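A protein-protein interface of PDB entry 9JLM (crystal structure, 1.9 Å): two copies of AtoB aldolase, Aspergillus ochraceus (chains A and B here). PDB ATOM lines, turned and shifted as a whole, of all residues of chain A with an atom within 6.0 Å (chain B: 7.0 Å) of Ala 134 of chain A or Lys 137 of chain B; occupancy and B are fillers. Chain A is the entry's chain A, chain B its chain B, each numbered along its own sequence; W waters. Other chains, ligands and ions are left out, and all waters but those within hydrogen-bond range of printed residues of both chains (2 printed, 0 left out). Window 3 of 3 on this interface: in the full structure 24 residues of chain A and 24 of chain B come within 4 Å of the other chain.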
ATOM      1  N   ASP A 132     -18.366  35.848   7.755  1.00  0.00           N
ATOM      2  CA  ASP A 132     -17.143  35.472   7.036  1.00  0.00           C
ATOM      3  C   ASP A 132     -16.256  34.675   7.997  1.00  0.00           C
ATOM      4  O   ASP A 132     -15.458  35.234   8.741  1.00  0.00           O
ATOM      5  CB  ASP A 132     -16.456  36.733   6.518  1.00  0.00           C
ATOM      6  CG  ASP A 132     -15.217  36.457   5.712  1.00  0.00           C
ATOM      7  OD1 ASP A 132     -14.685  35.337   5.794  1.00  0.00           O
ATOM      8  OD2 ASP A 132     -14.748  37.393   5.016  1.00  0.00           O
ATOM      9  N   THR A 133     -16.369  33.343   7.972  1.00  0.00           N
ATOM     10  CA  THR A 133     -15.756  32.545   9.036  1.00  0.00           C
ATOM     11  C   THR A 133     -14.227  32.647   9.047  1.00  0.00           C
ATOM     12  O   THR A 133     -13.614  32.678  10.124  1.00  0.00           O
ATOM     13  CB  THR A 133     -16.197  31.093   8.925  1.00  0.00           C
ATOM     14  OG1 THR A 133     -15.807  30.567   7.650  1.00  0.00           O
ATOM     15  CG2 THR A 133     -17.705  31.010   9.070  1.00  0.00           C
ATOM     16  N   ALA A 134     -13.587  32.704   7.875  1.00  0.00           N
ATOM     17  CA  ALA A 134     -12.136  32.880   7.852  1.00  0.00           C
ATOM     18  C   ALA A 134     -11.729  34.207   8.489  1.00  0.00           C
ATOM     19  O   ALA A 134     -10.773  34.268   9.271  1.00  0.00           O
ATOM     20  CB  ALA A 134     -11.614  32.785   6.420  1.00  0.00           C
ATOM     21  N   ALA A 135     -12.451  35.280   8.177  1.00  0.00           N
ATOM     22  CA  ALA A 135     -12.137  36.569   8.777  1.00  0.00           C
ATOM     23  C   ALA A 135     -12.360  36.551  10.287  1.00  0.00           C
ATOM     24  O   ALA A 135     -11.538  37.072  11.050  1.00  0.00           O
ATOM     25  CB  ALA A 135     -12.982  37.657   8.119  1.00  0.00           C
ATOM     26  N   GLU A 136     -13.474  35.956  10.733  1.00  0.00           N
ATOM     27  CA  GLU A 136     -13.845  36.027  12.144  1.00  0.00           C
ATOM     28  C   GLU A 136     -12.924  35.173  13.013  1.00  0.00           C
ATOM     29  O   GLU A 136     -12.585  35.564  14.138  1.00  0.00           O
ATOM     30  CB  GLU A 136     -15.302  35.600  12.306  1.00  0.00           C
ATOM     31  CG  GLU A 136     -16.276  36.512  11.580  1.00  0.00           C
ATOM     32  CD  GLU A 136     -16.399  37.895  12.218  1.00  0.00           C
ATOM     33  OE1 GLU A 136     -15.948  38.066  13.370  1.00  0.00           O
ATOM     34  OE2 GLU A 136     -16.942  38.815  11.562  1.00  0.00           O
ATOM     35  N   LYS A 137     -12.530  33.995  12.522  1.00  0.00           N
ATOM     36  CA  LYS A 137     -11.527  33.204  13.226  1.00  0.00           C
ATOM     37  C   LYS A 137     -10.233  33.994  13.390  1.00  0.00           C
ATOM     38  O   LYS A 137      -9.619  33.989  14.468  1.00  0.00           O
ATOM     39  CB  LYS A 137     -11.264  31.897  12.475  1.00  0.00           C
ATOM     40  CG  LYS A 137     -12.414  30.893  12.483  1.00  0.00           C
ATOM     41  CD  LYS A 137     -12.027  29.613  11.715  1.00  0.00           C
ATOM     42  CE  LYS A 137     -12.986  28.445  12.005  1.00  0.00           C
ATOM     43  NZ  LYS A 137     -14.367  28.621  11.429  1.00  0.00           N
ATOM     44  N   LYS A 138      -9.815  34.696  12.332  1.00  0.00           N
ATOM     45  CA  LYS A 138      -8.610  35.519  12.413  1.00  0.00           C
ATOM     46  C   LYS A 138      -8.774  36.629  13.447  1.00  0.00           C
ATOM     47  O   LYS A 138      -7.896  36.836  14.292  1.00  0.00           O
ATOM     48  CB  LYS A 138      -8.276  36.098  11.038  1.00  0.00           C
ATOM     49  CG  LYS A 138      -7.053  37.002  11.025  1.00  0.00           C
ATOM     50  CD  LYS A 138      -6.610  37.292   9.597  1.00  0.00           C
ATOM     51  CE  LYS A 138      -5.557  38.395   9.545  1.00  0.00           C
ATOM     52  NZ  LYS A 138      -5.216  38.753   8.135  1.00  0.00           N
ATOM     53  N   PHE A 139      -9.901  37.350  13.400  1.00  0.00           N
ATOM     54  CA  PHE A 139     -10.167  38.384  14.399  1.00  0.00           C
ATOM     55  C   PHE A 139     -10.146  37.804  15.813  1.00  0.00           C
ATOM     56  O   PHE A 139      -9.561  38.388  16.730  1.00  0.00           O
ATOM     57  CB  PHE A 139     -11.509  39.057  14.107  1.00  0.00           C
ATOM     58  CG  PHE A 139     -11.851  40.182  15.060  1.00  0.00           C
ATOM     59  CD1 PHE A 139     -11.359  41.459  14.851  1.00  0.00           C
ATOM     60  CD2 PHE A 139     -12.663  39.958  16.156  1.00  0.00           C
ATOM     61  CE1 PHE A 139     -11.666  42.486  15.714  1.00  0.00           C
ATOM     62  CE2 PHE A 139     -12.973  40.987  17.026  1.00  0.00           C
ATOM     63  CZ  PHE A 139     -12.471  42.251  16.803  1.00  0.00           C
ATOM     64  N   SER B  46     -14.372  38.630  -0.284  1.00  0.00           N
ATOM     65  CA  SER B  46     -13.071  38.345   0.318  1.00  0.00           C
ATOM     66  C   SER B  46     -12.610  36.939   0.010  1.00  0.00           C
ATOM     67  O   SER B  46     -11.406  36.671   0.048  1.00  0.00           O
ATOM     68  CB  SER B  46     -13.130  38.537   1.838  1.00  0.00           C
ATOM     69  OG  SER B  46     -13.911  37.506   2.434  1.00  0.00           O
ATOM     70  N   PHE B  47     -13.540  36.030  -0.284  1.00  0.00           N
ATOM     71  CA  PHE B  47     -13.143  34.693  -0.706  1.00  0.00           C
ATOM     72  C   PHE B  47     -12.420  34.712  -2.047  1.00  0.00           C
ATOM     73  O   PHE B  47     -11.679  33.774  -2.350  1.00  0.00           O
ATOM     74  CB  PHE B  47     -14.366  33.776  -0.761  1.00  0.00           C
ATOM     75  CG  PHE B  47     -14.041  32.341  -1.033  1.00  0.00           C
ATOM     76  CD1 PHE B  47     -13.300  31.599  -0.122  1.00  0.00           C
ATOM     77  CD2 PHE B  47     -14.502  31.719  -2.182  1.00  0.00           C
ATOM     78  CE1 PHE B  47     -13.006  30.274  -0.361  1.00  0.00           C
ATOM     79  CE2 PHE B  47     -14.214  30.391  -2.436  1.00  0.00           C
ATOM     80  CZ  PHE B  47     -13.462  29.664  -1.527  1.00  0.00           C
ATOM     81  N   GLY B  48     -12.603  35.760  -2.847  1.00  0.00           N
ATOM     82  CA  GLY B  48     -11.812  35.949  -4.049  1.00  0.00           C
ATOM     83  C   GLY B  48     -12.227  35.138  -5.259  1.00  0.00           C
ATOM     84  O   GLY B  48     -11.443  35.032  -6.208  1.00  0.00           O
ATOM     85  N   ASP B 132     -18.821  29.049   3.460  1.00  0.00           N
ATOM     86  CA  ASP B 132     -18.083  28.940   4.720  1.00  0.00           C
ATOM     87  C   ASP B 132     -16.603  29.114   4.385  1.00  0.00           C
ATOM     88  O   ASP B 132     -15.932  28.154   4.008  1.00  0.00           O
ATOM     89  CB  ASP B 132     -18.386  27.585   5.358  1.00  0.00           C
ATOM     90  CG  ASP B 132     -17.685  27.366   6.697  1.00  0.00           C
ATOM     91  OD1 ASP B 132     -16.713  28.085   7.019  1.00  0.00           O
ATOM     92  OD2 ASP B 132     -18.119  26.438   7.424  1.00  0.00           O
ATOM     93  N   THR B 133     -16.085  30.337   4.543  1.00  0.00           N
ATOM     94  CA  THR B 133     -14.789  30.682   3.945  1.00  0.00           C
ATOM     95  C   THR B 133     -13.618  29.989   4.638  1.00  0.00           C
ATOM     96  O   THR B 133     -12.630  29.639   3.983  1.00  0.00           O
ATOM     97  CB  THR B 133     -14.577  32.190   3.968  1.00  0.00           C
ATOM     98  OG1 THR B 133     -14.713  32.663   5.316  1.00  0.00           O
ATOM     99  CG2 THR B 133     -15.606  32.872   3.096  1.00  0.00           C
ATOM    100  N   ALA B 134     -13.682  29.815   5.959  1.00  0.00           N
ATOM    101  CA  ALA B 134     -12.642  29.051   6.641  1.00  0.00           C
ATOM    102  C   ALA B 134     -12.557  27.636   6.076  1.00  0.00           C
ATOM    103  O   ALA B 134     -11.471  27.151   5.734  1.00  0.00           O
ATOM    104  CB  ALA B 134     -12.921  29.022   8.146  1.00  0.00           C
ATOM    105  N   ALA B 135     -13.709  26.978   5.922  1.00  0.00           N
ATOM    106  CA  ALA B 135     -13.738  25.610   5.431  1.00  0.00           C
ATOM    107  C   ALA B 135     -13.460  25.539   3.935  1.00  0.00           C
ATOM    108  O   ALA B 135     -12.774  24.621   3.475  1.00  0.00           O
ATOM    109  CB  ALA B 135     -15.088  24.972   5.748  1.00  0.00           C
ATOM    110  N   GLU B 136     -13.986  26.484   3.147  1.00  0.00           N
ATOM    111  CA  GLU B 136     -13.715  26.430   1.709  1.00  0.00           C
ATOM    112  C   GLU B 136     -12.254  26.746   1.398  1.00  0.00           C
ATOM    113  O   GLU B 136     -11.716  26.243   0.407  1.00  0.00           O
ATOM    114  CB  GLU B 136     -14.641  27.375   0.931  1.00  0.00           C
ATOM    115  CG  GLU B 136     -16.143  27.068   1.039  1.00  0.00           C
ATOM    116  CD  GLU B 136     -16.566  25.756   0.392  1.00  0.00           C
ATOM    117  OE1 GLU B 136     -15.762  25.127  -0.309  1.00  0.00           O
ATOM    118  OE2 GLU B 136     -17.726  25.343   0.587  1.00  0.00           O
ATOM    119  N   LYS B 137     -11.589  27.561   2.226  1.00  0.00           N
ATOM    120  CA  LYS B 137     -10.163  27.815   2.004  1.00  0.00           C
ATOM    121  C   LYS B 137      -9.320  26.596   2.370  1.00  0.00           C
ATOM    122  O   LYS B 137      -8.383  26.240   1.640  1.00  0.00           O
ATOM    123  CB  LYS B 137      -9.701  29.045   2.795  1.00  0.00           C
ATOM    124  CG  LYS B 137     -10.204  30.391   2.252  1.00  0.00           C
ATOM    125  CD  LYS B 137      -9.496  31.559   2.945  1.00  0.00           C
ATOM    126  CE  LYS B 137     -10.348  32.839   2.983  1.00  0.00           C
ATOM    127  NZ  LYS B 137     -10.212  33.720   1.777  1.00  0.00           N
ATOM    128  N   LYS B 138      -9.620  25.966   3.512  1.00  0.00           N
ATOM    129  CA  LYS B 138      -9.028  24.680   3.867  1.00  0.00           C
ATOM    130  C   LYS B 138      -9.140  23.694   2.707  1.00  0.00           C
ATOM    131  O   LYS B 138      -8.132  23.223   2.165  1.00  0.00           O
ATOM    132  CB  LYS B 138      -9.725  24.127   5.113  1.00  0.00           C
ATOM    133  CG  LYS B 138      -8.879  23.201   5.975  1.00  0.00           C
ATOM    134  CD  LYS B 138      -9.512  21.822   6.122  1.00  0.00           C
ATOM    135  CE  LYS B 138      -8.838  21.008   7.236  1.00  0.00           C
ATOM    136  NZ  LYS B 138      -9.271  19.568   7.284  1.00  0.00           N
ATOM    137  N   PHE B 139     -10.379  23.398   2.305  1.00  0.00           N
ATOM    138  CA  PHE B 139     -10.652  22.483   1.199  1.00  0.00           C
ATOM    139  C   PHE B 139      -9.833  22.830  -0.047  1.00  0.00           C
ATOM    140  O   PHE B 139      -9.199  21.957  -0.653  1.00  0.00           O
ATOM    141  CB  PHE B 139     -12.156  22.511   0.895  1.00  0.00           C
ATOM    142  CG  PHE B 139     -12.594  21.519  -0.140  1.00  0.00           C
ATOM    143  CD1 PHE B 139     -12.479  20.160   0.091  1.00  0.00           C
ATOM    144  CD2 PHE B 139     -13.146  21.946  -1.335  1.00  0.00           C
ATOM    145  CE1 PHE B 139     -12.890  19.247  -0.863  1.00  0.00           C
ATOM    146  CE2 PHE B 139     -13.561  21.038  -2.289  1.00  0.00           C
ATOM    147  CZ  PHE B 139     -13.430  19.688  -2.051  1.00  0.00           C
ATOM    148  N   ALA B 140      -9.839  24.106  -0.445  1.00  0.00           N
ATOM    149  CA  ALA B 140      -9.090  24.520  -1.625  1.00  0.00           C
ATOM    150  C   ALA B 140      -7.586  24.378  -1.414  1.00  0.00           C
ATOM    151  O   ALA B 140      -6.848  24.095  -2.366  1.00  0.00           O
ATOM    152  CB  ALA B 140      -9.449  25.961  -1.996  1.00  0.00           C
ATOM    153  N   ALA B 141      -7.115  24.560  -0.182  1.00  0.00           N
ATOM    154  CA  ALA B 141      -5.698  24.363   0.096  1.00  0.00           C
ATOM    155  C   ALA B 141      -5.337  22.883   0.093  1.00  0.00           C
ATOM    156  O   ALA B 141      -4.244  22.509  -0.348  1.00  0.00           O
ATOM    157  CB  ALA B 141      -5.327  25.003   1.431  1.00  0.00           C
ATOM    158  N   GLU B 142      -6.239  22.026   0.586  1.00  0.00           N
ATOM    159  CA  GLU B 142      -5.960  20.593   0.605  1.00  0.00           C
ATOM    160  C   GLU B 142      -5.767  20.040  -0.805  1.00  0.00           C
ATOM    161  O   GLU B 142      -5.053  19.047  -0.988  1.00  0.00           O
ATOM    162  CB  GLU B 142      -7.081  19.839   1.327  1.00  0.00           C
ATOM    163  CG  GLU B 142      -7.185  20.096   2.838  1.00  0.00           C
ATOM    164  CD  GLU B 142      -8.408  19.419   3.458  1.00  0.00           C
ATOM    165  OE1 GLU B 142      -9.363  19.123   2.708  1.00  0.00           O
ATOM    166  OE2 GLU B 142      -8.426  19.170   4.686  1.00  0.00           O
ATOM    167  N   ARG B 143      -6.371  20.672  -1.808  1.00  0.00           N
ATOM    168  CA  ARG B 143      -6.243  20.209  -3.186  1.00  0.00           C
ATOM    169  C   ARG B 143      -5.030  20.827  -3.875  1.00  0.00           C
ATOM    170  O   ARG B 143      -4.017  20.159  -4.083  1.00  0.00           O
ATOM    171  CB  ARG B 143      -7.514  20.520  -3.980  1.00  0.00           C
ATOM    172  CG  ARG B 143      -8.765  19.840  -3.443  1.00  0.00           C
ATOM    173  CD  ARG B 143      -8.567  18.329  -3.255  1.00  0.00           C
ATOM    174  NE  ARG B 143      -8.390  17.601  -4.514  1.00  0.00           N
ATOM    175  CZ  ARG B 143      -7.292  16.927  -4.850  1.00  0.00           C
ATOM    176  NH1 ARG B 143      -6.258  16.877  -4.019  1.00  0.00           N
ATOM    177  NH2 ARG B 143      -7.227  16.294  -6.014  1.00  0.00           N
HETATM  178  O   HOH W   1     -15.543  27.383   9.569  1.00  0.00           O
HETATM  179  O   HOH W   2     -17.963  32.338   5.758  1.00  0.00           O
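Water W1 bridges NZ of Lys 137 of chain A (2.5 Å) and OD1 of Asp 132 of chain B (2.9 Å). Water W2 bridges N of Thr 133 of chain A (2.9 Å) and N of Thr 133 of chain B (3.0 Å).
Among the printed residues, pairs that only touch across the chains: Ala 134 of chain A with Lys 137 of chain B (3.7 Å) and Lys 137 of chain A with Ala 134 of chain B (3.6 Å).
Thr 133 of chain B touches its own counterpart, Thr 133 of chain A. Thr 133 of chain A touches Ala 134 of chain B, and with the chains exchanged Ala 134 of chain A touches Thr 133 of chain B. Ala 134 of chain B touches its own counterpart, Ala 134 of chain A. Ala 134 of chain A touches Lys 137 of chain B, and with the chains exchanged Lys 137 of chain A touches Ala 134 of chain B.
The side-chain hydroxyl of Thr 133 of chain B is in hydrogen-bond range of the side-chain carboxylate of Asp 132 of chain A (2.7 Å). The side-chain hydroxyl of Thr 133 of chain A lies within hydrogen-bond range of the side-chain carboxylate of Asp 132 of chain B (2.7 Å). The side-chain hydroxyl (OG1) of Thr 133 of chain B is in hydrogen-bond range of the backbone NH (N) of Ala 134 of chain A (2.8 Å). The backbone NH (N) of Ala 134 of chain A sits close to the backbone NH (N) of Ala 134 of chain B (3.5 Å). The side-chain hydroxyl of Ser 46 of chain B sits at hydrogen-bond distance from the side-chain carboxylate of Asp 132 of chain A (2.7 Å). The side-chain hydroxyl (OG1) of Thr 133 of chain A is in hydrogen-bond range of the backbone NH (N) of Ala 134 of chain B (2.8 Å). OG1 of Thr 133 of chain A sits at hydrogen-bond distance from N of Thr 133 of chain B, at 3.1 Å.
Of the 8 printed residues of chain A, 4 touch a printed residue of chain B. Hydrophobic or aromatic side chains of chain A within 4 Å of the printed part of chain B: Ala 134. Hydrophobic or aromatic side chains of chain B within 4 Å of the printed part of chain A: Ala 134. Among the printed residues, 9 pairs touch across the chains. Among the printed residues, no Asp or Glu carboxylate lies within 4 Å of a Lys or Arg side-chain nitrogen of the other chain.
Printed residues of chain B within 4 Å of Asp 132 of chain A: Ser 46 (2.7 Å) and Thr 133 (2.7 Å). Of chain B, only Thr 133, Ala 134 and Lys 137 come within 4 Å of Ala 134 of chain A. Printed residues of chain B within 4 Å of Lys 137 of chain A: Ala 134. Of the printed residues of chain A, Ser 46 of chain B touches Asp 132. Phe 47 of chain B touches none of the printed residues of chain A. Printed residues of chain A within 4 Å of Asp 132 of chain B: Thr 133 (2.7 Å). Of the printed residues of chain A, Thr 133 of chain B touches Asp 132, Thr 133 and Ala 134. Lys 137 of chain B touches just one residue of chain A: Ala 134. Ala 140 of chain B touches none of the printed residues of chain A. The nearest printed residue of chain A that does not touch Ser 46 of chain B is Ala 135 of chain A (5.8 Å).
The side-chain carboxylate of Asp 132 of chain A sits at hydrogen-bond distance from the backbone NH of Ala 135 of chain A, 3.3 Å away. N of Ala 135 of chain B is in hydrogen-bond range of OD1 of Asp 132 of chain B.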
